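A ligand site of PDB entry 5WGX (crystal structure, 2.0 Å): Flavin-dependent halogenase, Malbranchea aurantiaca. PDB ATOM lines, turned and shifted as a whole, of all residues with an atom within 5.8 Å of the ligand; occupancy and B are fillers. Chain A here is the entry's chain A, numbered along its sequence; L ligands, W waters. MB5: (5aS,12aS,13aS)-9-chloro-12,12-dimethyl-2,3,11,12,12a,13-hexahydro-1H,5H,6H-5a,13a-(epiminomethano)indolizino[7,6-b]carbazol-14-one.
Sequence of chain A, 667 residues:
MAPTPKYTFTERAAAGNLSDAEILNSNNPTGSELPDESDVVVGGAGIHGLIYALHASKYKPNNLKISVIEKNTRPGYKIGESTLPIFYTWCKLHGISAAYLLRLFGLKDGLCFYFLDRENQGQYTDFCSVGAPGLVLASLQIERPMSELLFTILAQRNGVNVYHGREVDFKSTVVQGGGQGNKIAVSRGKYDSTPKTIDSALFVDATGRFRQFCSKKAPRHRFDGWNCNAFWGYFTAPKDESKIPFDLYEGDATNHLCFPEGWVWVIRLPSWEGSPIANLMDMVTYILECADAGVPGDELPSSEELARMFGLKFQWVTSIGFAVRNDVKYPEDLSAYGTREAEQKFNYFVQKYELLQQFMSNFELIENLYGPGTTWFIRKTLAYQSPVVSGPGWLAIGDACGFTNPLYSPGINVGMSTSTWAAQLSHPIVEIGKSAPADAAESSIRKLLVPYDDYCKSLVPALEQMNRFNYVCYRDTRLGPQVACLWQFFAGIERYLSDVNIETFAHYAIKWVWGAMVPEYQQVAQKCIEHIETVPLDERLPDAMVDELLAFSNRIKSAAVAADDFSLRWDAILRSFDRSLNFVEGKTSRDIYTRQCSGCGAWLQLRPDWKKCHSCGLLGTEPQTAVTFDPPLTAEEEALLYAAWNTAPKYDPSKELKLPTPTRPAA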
ATOM      1  N   PRO A  85     -13.360  11.272   6.207  1.00  0.00           N
ATOM      2  CA  PRO A  85     -12.229  12.006   5.606  1.00  0.00           C
ATOM      3  C   PRO A  85     -12.307  12.190   4.099  1.00  0.00           C
ATOM      4  O   PRO A  85     -11.875  13.237   3.603  1.00  0.00           O
ATOM      5  CB  PRO A  85     -11.024  11.139   6.001  1.00  0.00           C
ATOM      6  CG  PRO A  85     -11.427  10.563   7.333  1.00  0.00           C
ATOM      7  CD  PRO A  85     -12.901  10.321   7.241  1.00  0.00           C
ATOM      8  N   LEU A 111     -14.553   7.384  15.274  1.00  0.00           N
ATOM      9  CA  LEU A 111     -15.717   6.516  15.323  1.00  0.00           C
ATOM     10  C   LEU A 111     -15.564   5.649  16.565  1.00  0.00           C
ATOM     11  O   LEU A 111     -14.602   4.875  16.665  1.00  0.00           O
ATOM     12  CB  LEU A 111     -15.829   5.659  14.071  1.00  0.00           C
ATOM     13  CG  LEU A 111     -16.244   6.337  12.754  1.00  0.00           C
ATOM     14  CD1 LEU A 111     -15.082   7.104  12.158  1.00  0.00           C
ATOM     15  CD2 LEU A 111     -16.768   5.301  11.792  1.00  0.00           C
ATOM     16  N   SER A 129     -11.537   5.131  18.593  1.00  0.00           N
ATOM     17  CA  SER A 129     -10.605   5.615  17.587  1.00  0.00           C
ATOM     18  C   SER A 129     -10.638   7.130  17.568  1.00  0.00           C
ATOM     19  O   SER A 129     -11.590   7.767  18.015  1.00  0.00           O
ATOM     20  CB  SER A 129     -10.923   5.068  16.188  1.00  0.00           C
ATOM     21  OG  SER A 129     -12.096   5.653  15.667  1.00  0.00           O
ATOM     22  N   VAL A 130      -9.567   7.714  17.024  1.00  0.00           N
ATOM     23  CA  VAL A 130      -9.437   9.158  16.919  1.00  0.00           C
ATOM     24  C   VAL A 130      -9.471   9.534  15.444  1.00  0.00           C
ATOM     25  O   VAL A 130      -9.400   8.698  14.552  1.00  0.00           O
ATOM     26  CB  VAL A 130      -8.159   9.670  17.598  1.00  0.00           C
ATOM     27  CG1 VAL A 130      -8.181   9.336  19.084  1.00  0.00           C
ATOM     28  CG2 VAL A 130      -6.932   9.071  16.917  1.00  0.00           C
ATOM     29  N   GLY A 131      -9.598  10.841  15.190  1.00  0.00           N
ATOM     30  CA  GLY A 131      -9.526  11.359  13.838  1.00  0.00           C
ATOM     31  C   GLY A 131      -8.114  11.752  13.460  1.00  0.00           C
ATOM     32  O   GLY A 131      -7.216  10.906  13.424  1.00  0.00           O
ATOM     33  N   ALA A 132      -7.887  13.040  13.211  1.00  0.00           N
ATOM     34  CA  ALA A 132      -6.602  13.542  12.756  1.00  0.00           C
ATOM     35  C   ALA A 132      -6.317  14.871  13.437  1.00  0.00           C
ATOM     36  O   ALA A 132      -7.254  15.541  13.902  1.00  0.00           O
ATOM     37  CB  ALA A 132      -6.579  13.715  11.230  1.00  0.00           C
ATOM     38  N   PRO A 133      -5.048  15.275  13.528  1.00  0.00           N
ATOM     39  CA  PRO A 133      -4.741  16.616  14.031  1.00  0.00           C
ATOM     40  C   PRO A 133      -5.420  17.690  13.183  1.00  0.00           C
ATOM     41  O   PRO A 133      -5.713  17.492  12.007  1.00  0.00           O
ATOM     42  CB  PRO A 133      -3.218  16.700  13.920  1.00  0.00           C
ATOM     43  CG  PRO A 133      -2.763  15.288  13.977  1.00  0.00           C
ATOM     44  CD  PRO A 133      -3.836  14.479  13.288  1.00  0.00           C
ATOM     45  N   VAL A 136      -3.961  18.342   9.944  1.00  0.00           N
ATOM     46  CA  VAL A 136      -3.966  17.245   8.984  1.00  0.00           C
ATOM     47  C   VAL A 136      -5.293  17.276   8.215  1.00  0.00           C
ATOM     48  O   VAL A 136      -5.301  17.537   7.008  1.00  0.00           O
ATOM     49  CB  VAL A 136      -3.751  15.898   9.672  1.00  0.00           C
ATOM     50  CG1 VAL A 136      -3.951  14.754   8.682  1.00  0.00           C
ATOM     51  CG2 VAL A 136      -2.362  15.843  10.281  1.00  0.00           C
ATOM     52  N   LEU A 137      -6.393  17.013   8.902  1.00  0.00           N
ATOM     53  CA  LEU A 137      -7.719  17.112   8.305  1.00  0.00           C
ATOM     54  C   LEU A 137      -8.769  17.122   9.419  1.00  0.00           C
ATOM     55  O   LEU A 137      -8.447  17.008  10.609  1.00  0.00           O
ATOM     56  CB  LEU A 137      -7.986  15.964   7.312  1.00  0.00           C
ATOM     57  CG  LEU A 137      -7.990  14.494   7.772  1.00  0.00           C
ATOM     58  CD1 LEU A 137      -9.295  14.078   8.467  1.00  0.00           C
ATOM     59  CD2 LEU A 137      -7.716  13.583   6.579  1.00  0.00           C
ATOM     60  N   TYR A 408     -21.423   3.188   9.600  1.00  0.00           N
ATOM     61  CA  TYR A 408     -20.184   3.612   8.936  1.00  0.00           C
ATOM     62  C   TYR A 408     -20.437   4.625   7.835  1.00  0.00           C
ATOM     63  O   TYR A 408     -19.520   4.926   7.068  1.00  0.00           O
ATOM     64  CB  TYR A 408     -19.372   2.421   8.382  1.00  0.00           C
ATOM     65  CG  TYR A 408     -18.672   1.660   9.466  1.00  0.00           C
ATOM     66  CD1 TYR A 408     -17.535   2.177  10.068  1.00  0.00           C
ATOM     67  CD2 TYR A 408     -19.163   0.451   9.942  1.00  0.00           C
ATOM     68  CE1 TYR A 408     -16.880   1.502  11.079  1.00  0.00           C
ATOM     69  CE2 TYR A 408     -18.526  -0.233  10.963  1.00  0.00           C
ATOM     70  CZ  TYR A 408     -17.383   0.294  11.525  1.00  0.00           C
ATOM     71  OH  TYR A 408     -16.739  -0.367  12.538  1.00  0.00           O
ATOM     72  N   GLN A 488     -13.058  -3.512   9.891  1.00  0.00           N
ATOM     73  CA  GLN A 488     -13.532  -2.373   9.116  1.00  0.00           C
ATOM     74  C   GLN A 488     -12.484  -1.257   9.093  1.00  0.00           C
ATOM     75  O   GLN A 488     -12.301  -0.584   8.073  1.00  0.00           O
ATOM     76  CB  GLN A 488     -14.846  -1.847   9.679  1.00  0.00           C
ATOM     77  CG  GLN A 488     -15.648  -1.039   8.675  1.00  0.00           C
ATOM     78  CD  GLN A 488     -16.298  -1.934   7.637  1.00  0.00           C
ATOM     79  OE1 GLN A 488     -17.103  -2.797   7.976  1.00  0.00           O
ATOM     80  NE2 GLN A 488     -15.951  -1.728   6.374  1.00  0.00           N
ATOM     81  N   PHE A 489     -11.806  -1.058  10.216  1.00  0.00           N
ATOM     82  CA  PHE A 489     -10.790  -0.013  10.282  1.00  0.00           C
ATOM     83  C   PHE A 489      -9.548  -0.400   9.487  1.00  0.00           C
ATOM     84  O   PHE A 489      -9.000   0.430   8.746  1.00  0.00           O
ATOM     85  CB  PHE A 489     -10.443   0.284  11.739  1.00  0.00           C
ATOM     86  CG  PHE A 489     -11.474   1.120  12.462  1.00  0.00           C
ATOM     87  CD1 PHE A 489     -12.805   0.732  12.484  1.00  0.00           C
ATOM     88  CD2 PHE A 489     -11.107   2.268  13.137  1.00  0.00           C
ATOM     89  CE1 PHE A 489     -13.761   1.480  13.142  1.00  0.00           C
ATOM     90  CE2 PHE A 489     -12.059   3.035  13.801  1.00  0.00           C
ATOM     91  CZ  PHE A 489     -13.389   2.641  13.807  1.00  0.00           C
ATOM     92  N   GLY A 492     -10.552  -0.578   5.702  1.00  0.00           N
ATOM     93  CA  GLY A 492     -11.174   0.604   5.139  1.00  0.00           C
ATOM     94  C   GLY A 492     -10.474   1.922   5.364  1.00  0.00           C
ATOM     95  O   GLY A 492     -10.931   2.946   4.863  1.00  0.00           O
ATOM     96  N   ILE A 493      -9.379   1.930   6.134  1.00  0.00           N
ATOM     97  CA  ILE A 493      -8.675   3.186   6.351  1.00  0.00           C
ATOM     98  C   ILE A 493      -8.118   3.678   5.019  1.00  0.00           C
ATOM     99  O   ILE A 493      -7.669   2.891   4.174  1.00  0.00           O
ATOM    100  CB  ILE A 493      -7.572   3.021   7.416  1.00  0.00           C
ATOM    101  CG1 ILE A 493      -6.971   4.382   7.771  1.00  0.00           C
ATOM    102  CG2 ILE A 493      -6.492   2.050   6.975  1.00  0.00           C
ATOM    103  CD1 ILE A 493      -6.303   4.411   9.123  1.00  0.00           C
ATOM    104  N   GLU A 494      -8.173   4.993   4.820  1.00  0.00           N
ATOM    105  CA  GLU A 494      -7.996   5.610   3.514  1.00  0.00           C
ATOM    106  C   GLU A 494      -6.512   5.864   3.258  1.00  0.00           C
ATOM    107  O   GLU A 494      -6.003   6.981   3.385  1.00  0.00           O
ATOM    108  CB  GLU A 494      -8.800   6.899   3.417  1.00  0.00           C
ATOM    109  CG  GLU A 494     -10.287   6.728   3.760  1.00  0.00           C
ATOM    110  CD  GLU A 494     -10.615   7.030   5.219  1.00  0.00           C
ATOM    111  OE1 GLU A 494      -9.725   6.880   6.092  1.00  0.00           O
ATOM    112  OE2 GLU A 494     -11.768   7.413   5.496  1.00  0.00           O
ATOM    113  N   ARG A 495      -5.812   4.807   2.863  1.00  0.00           N
ATOM    114  CA  ARG A 495      -4.385   4.909   2.590  1.00  0.00           C
ATOM    115  C   ARG A 495      -4.141   5.811   1.386  1.00  0.00           C
ATOM    116  O   ARG A 495      -4.840   5.724   0.376  1.00  0.00           O
ATOM    117  CB  ARG A 495      -3.778   3.523   2.343  1.00  0.00           C
ATOM    118  CG  ARG A 495      -3.865   2.579   3.549  1.00  0.00           C
ATOM    119  CD  ARG A 495      -3.581   1.138   3.150  1.00  0.00           C
ATOM    120  NE  ARG A 495      -3.640   0.226   4.295  1.00  0.00           N
ATOM    121  CZ  ARG A 495      -4.767  -0.250   4.814  1.00  0.00           C
ATOM    122  NH1 ARG A 495      -5.939   0.101   4.286  1.00  0.00           N
ATOM    123  NH2 ARG A 495      -4.728  -1.072   5.854  1.00  0.00           N
ATOM    124  N   LEU A 497      -4.660   8.959   1.015  1.00  0.00           N
ATOM    125  CA  LEU A 497      -5.676   9.982   0.765  1.00  0.00           C
ATOM    126  C   LEU A 497      -5.040  11.338   0.506  1.00  0.00           C
ATOM    127  O   LEU A 497      -5.585  12.141  -0.267  1.00  0.00           O
ATOM    128  CB  LEU A 497      -6.633  10.052   1.959  1.00  0.00           C
ATOM    129  CG  LEU A 497      -7.768  11.081   1.988  1.00  0.00           C
ATOM    130  CD1 LEU A 497      -8.779  10.801   0.889  1.00  0.00           C
ATOM    131  CD2 LEU A 497      -8.436  11.067   3.360  1.00  0.00           C
ATOM    132  N   TRP A 514     -15.120   1.436   1.524  1.00  0.00           N
ATOM    133  CA  TRP A 514     -14.934   1.202   2.960  1.00  0.00           C
ATOM    134  C   TRP A 514     -14.137  -0.072   3.236  1.00  0.00           C
ATOM    135  O   TRP A 514     -14.248  -0.655   4.324  1.00  0.00           O
ATOM    136  CB  TRP A 514     -16.277   1.161   3.693  1.00  0.00           C
ATOM    137  CG  TRP A 514     -16.502   2.280   4.672  1.00  0.00           C
ATOM    138  CD1 TRP A 514     -17.493   3.228   4.627  1.00  0.00           C
ATOM    139  CD2 TRP A 514     -15.713   2.568   5.833  1.00  0.00           C
ATOM    140  NE1 TRP A 514     -17.362   4.089   5.699  1.00  0.00           N
ATOM    141  CE2 TRP A 514     -16.278   3.708   6.450  1.00  0.00           C
ATOM    142  CE3 TRP A 514     -14.585   1.991   6.408  1.00  0.00           C
ATOM    143  CZ2 TRP A 514     -15.759   4.267   7.622  1.00  0.00           C
ATOM    144  CZ3 TRP A 514     -14.061   2.540   7.571  1.00  0.00           C
ATOM    145  CH2 TRP A 514     -14.649   3.673   8.161  1.00  0.00           C
ATOM    146  N   LEU A 568       1.734   3.168   9.722  1.00  0.00           N
ATOM    147  CA  LEU A 568       0.652   3.780  10.484  1.00  0.00           C
ATOM    148  C   LEU A 568       0.884   3.533  11.959  1.00  0.00           C
ATOM    149  O   LEU A 568       1.137   2.394  12.374  1.00  0.00           O
ATOM    150  CB  LEU A 568      -0.698   3.195  10.050  1.00  0.00           C
ATOM    151  CG  LEU A 568      -1.915   4.089   9.873  1.00  0.00           C
ATOM    152  CD1 LEU A 568      -1.535   5.504   9.492  1.00  0.00           C
ATOM    153  CD2 LEU A 568      -2.810   3.494   8.798  1.00  0.00           C
ATOM    154  N   ILE A 573      -3.842   5.554  17.090  1.00  0.00           N
ATOM    155  CA  ILE A 573      -5.157   5.798  16.502  1.00  0.00           C
ATOM    156  C   ILE A 573      -6.236   4.981  17.198  1.00  0.00           C
ATOM    157  O   ILE A 573      -7.357   5.462  17.401  1.00  0.00           O
ATOM    158  CB  ILE A 573      -5.113   5.498  14.998  1.00  0.00           C
ATOM    159  CG1 ILE A 573      -4.008   6.311  14.333  1.00  0.00           C
ATOM    160  CG2 ILE A 573      -6.466   5.780  14.349  1.00  0.00           C
ATOM    161  CD1 ILE A 573      -3.633   5.825  12.952  1.00  0.00           C
ATOM    162  N   LEU A 574      -5.936   3.736  17.564  1.00  0.00           N
ATOM    163  CA  LEU A 574      -6.881   2.840  18.222  1.00  0.00           C
ATOM    164  C   LEU A 574      -6.458   2.668  19.674  1.00  0.00           C
ATOM    165  O   LEU A 574      -5.338   2.209  19.955  1.00  0.00           O
ATOM    166  CB  LEU A 574      -6.943   1.489  17.528  1.00  0.00           C
ATOM    167  CG  LEU A 574      -7.320   1.476  16.042  1.00  0.00           C
ATOM    168  CD1 LEU A 574      -7.491   0.049  15.565  1.00  0.00           C
ATOM    169  CD2 LEU A 574      -8.586   2.292  15.810  1.00  0.00           C
ATOM    170  N   TYR A 593      -6.466  14.986  19.811  1.00  0.00           N
ATOM    171  CA  TYR A 593      -6.512  16.020  18.786  1.00  0.00           C
ATOM    172  C   TYR A 593      -7.541  17.110  19.066  1.00  0.00           C
ATOM    173  O   TYR A 593      -7.565  18.108  18.336  1.00  0.00           O
ATOM    174  CB  TYR A 593      -6.838  15.400  17.427  1.00  0.00           C
ATOM    175  CG  TYR A 593      -5.901  14.309  16.973  1.00  0.00           C
ATOM    176  CD1 TYR A 593      -4.533  14.388  17.209  1.00  0.00           C
ATOM    177  CD2 TYR A 593      -6.393  13.192  16.304  1.00  0.00           C
ATOM    178  CE1 TYR A 593      -3.677  13.385  16.782  1.00  0.00           C
ATOM    179  CE2 TYR A 593      -5.552  12.183  15.874  1.00  0.00           C
ATOM    180  CZ  TYR A 593      -4.193  12.285  16.114  1.00  0.00           C
ATOM    181  OH  TYR A 593      -3.354  11.273  15.697  1.00  0.00           O
ATOM    182  N   LEU A 641       4.528  15.317   9.198  1.00  0.00           N
ATOM    183  CA  LEU A 641       3.130  14.919   9.091  1.00  0.00           C
ATOM    184  C   LEU A 641       2.282  16.054   8.524  1.00  0.00           C
ATOM    185  O   LEU A 641       1.514  15.861   7.574  1.00  0.00           O
ATOM    186  CB  LEU A 641       2.597  14.494  10.465  1.00  0.00           C
ATOM    187  CG  LEU A 641       1.111  14.188  10.643  1.00  0.00           C
ATOM    188  CD1 LEU A 641       0.674  13.033   9.758  1.00  0.00           C
ATOM    189  CD2 LEU A 641       0.813  13.884  12.093  1.00  0.00           C
ATOM    190  N   TRP A 645       0.013  17.028   4.341  1.00  0.00           N
ATOM    191  CA  TRP A 645      -1.414  17.294   4.229  1.00  0.00           C
ATOM    192  C   TRP A 645      -1.715  18.761   3.949  1.00  0.00           C
ATOM    193  O   TRP A 645      -2.885  19.172   4.031  1.00  0.00           O
ATOM    194  CB  TRP A 645      -2.136  16.851   5.500  1.00  0.00           C
ATOM    195  CG  TRP A 645      -2.134  15.365   5.670  1.00  0.00           C
ATOM    196  CD1 TRP A 645      -1.177  14.607   6.281  1.00  0.00           C
ATOM    197  CD2 TRP A 645      -3.140  14.452   5.206  1.00  0.00           C
ATOM    198  NE1 TRP A 645      -1.528  13.285   6.240  1.00  0.00           N
ATOM    199  CE2 TRP A 645      -2.728  13.164   5.583  1.00  0.00           C
ATOM    200  CE3 TRP A 645      -4.340  14.611   4.509  1.00  0.00           C
ATOM    201  CZ2 TRP A 645      -3.484  12.021   5.284  1.00  0.00           C
ATOM    202  CZ3 TRP A 645      -5.088  13.474   4.220  1.00  0.00           C
ATOM    203  CH2 TRP A 645      -4.652  12.197   4.610  1.00  0.00           C
HETATM  204  N   MB5 L   1      -5.251  10.334  11.376  1.00  0.00           N
HETATM  205  C   MB5 L   1      -4.216  10.995  10.818  1.00  0.00           C
HETATM  206  O   MB5 L   1      -3.696  11.970  11.322  1.00  0.00           O
HETATM  207  C1  MB5 L   1      -3.794  10.398   9.481  1.00  0.00           C
HETATM  208  C10 MB5 L   1     -10.978   5.046  10.692  1.00  0.00           C
HETATM  209  C11 MB5 L   1     -10.556   5.588   9.495  1.00  0.00           C
HETATM  210  C12 MB5 L   1      -9.529   6.511   9.531  1.00  0.00           C
HETATM  211  C13 MB5 L   1      -7.944   8.032   9.062  1.00  0.00           C
HETATM  212  C14 MB5 L   1      -7.048   8.930   8.252  1.00  0.00           C
HETATM  213  C15 MB5 L   1      -6.195   8.047   7.333  1.00  0.00           C
HETATM  214  C16 MB5 L   1      -7.929   9.824   7.355  1.00  0.00           C
HETATM  215  C17 MB5 L   1      -4.584   8.244  10.423  1.00  0.00           C
HETATM  216  C18 MB5 L   1      -2.205   9.008  10.338  1.00  0.00           C
HETATM  217  C19 MB5 L   1      -1.422   9.964   9.468  1.00  0.00           C
HETATM  218  C2  MB5 L   1      -5.014  10.514   8.542  1.00  0.00           C
HETATM  219  C20 MB5 L   1      -2.462  10.945   8.940  1.00  0.00           C
HETATM  220  C3  MB5 L   1      -6.206   9.815   9.224  1.00  0.00           C
HETATM  221  C4  MB5 L   1      -5.771   9.198  10.610  1.00  0.00           C
HETATM  222  C5  MB5 L   1      -7.006   8.618  11.332  1.00  0.00           C
HETATM  223  C6  MB5 L   1      -7.912   7.861  10.420  1.00  0.00           C
HETATM  224  C7  MB5 L   1      -8.922   6.894  10.750  1.00  0.00           C
HETATM  225  C8  MB5 L   1      -9.374   6.321  11.929  1.00  0.00           C
HETATM  226  C9  MB5 L   1     -10.409   5.399  11.899  1.00  0.00           C
HETATM  227  N1  MB5 L   1      -8.916   7.221   8.511  1.00  0.00           N
HETATM  228  N2  MB5 L   1      -3.532   8.960   9.697  1.00  0.00           N
HETATM  229 CL   MB5 L   1     -12.281   3.879  10.676  1.00  0.00          CL
HETATM  230  O   HOH W   1      -1.806  11.400  13.425  1.00  0.00           O
HETATM  231  O   HOH W   2     -12.947   6.843   7.895  1.00  0.00           O
HETATM  232  O   HOH W   3     -12.435   8.280  10.051  1.00  0.00           O
HETATM  233  O   HOH W   4     -11.697   8.419  12.829  1.00  0.00           O
HETATM  234  O   HOH W   5       0.393   7.321  11.650  1.00  0.00           O
HETATM  235  O   HOH W   6      -2.736   7.888   7.164  1.00  0.00           O
HETATM  236  O   HOH W   7      -9.954  10.235  10.508  1.00  0.00           O
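OE1 of Glu 494 sits at hydrogen-bond distance from N1 of the ligand (2.6 Å). O of Gly 131 sits at hydrogen-bond distance from N of the ligand (2.9 Å).
The side-chain amide nitrogen (NE2) of Gln 488 sits at hydrogen-bond distance from the backbone carbonyl oxygen (O) of Trp 514, at 2.9 Å. The indole nitrogen of Trp 514 lies within hydrogen-bond range of the backbone carbonyl oxygen of Tyr 408 (2.7 Å). The backbone carbonyl oxygen of Ile 493 is in hydrogen-bond range of the guanidinium group of Arg 495. The backbone NH (N) of Val 130 sits at hydrogen-bond distance from the backbone carbonyl oxygen (O) of Ile 573 (3.2 Å).
Merely in contact with the ligand: Pro 85 (3.6 Å), Val 130 (3.5 Å), Ala 132 (3.4 Å), Pro 133 (3.2 Å), Val 136 (3.8 Å), Leu 137 (3.8 Å), Phe 489 (3.2 Å), Ile 493 (3.5 Å), Trp 514 (3.5 Å), Leu 568 (3.7 Å), Ile 573 (3.6 Å), Leu 641 (3.7 Å) and Trp 645 (3.7 Å). Hydrophobic or aromatic side chains that line the ligand: Pro 85, Ala 132, Pro 133, Val 136, Leu 137, Phe 489, Ile 493, Trp 514, Leu 568, Ile 573, Leu 641 and Trp 645. 15 residues have an atom within 4 Å of the ligand: Pro 85, Val 130, Gly 131, Ala 132, Pro 133, Val 136, Leu 137, Phe 489, Ile 493, Glu 494, Trp 514, Leu 568, Ile 573, Leu 641 and Trp 645. The nearest printed residue that does not touch the ligand is Ser 129 (4.1 Å).
Water W1 bridges OH of Tyr 593 and O of the ligand.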
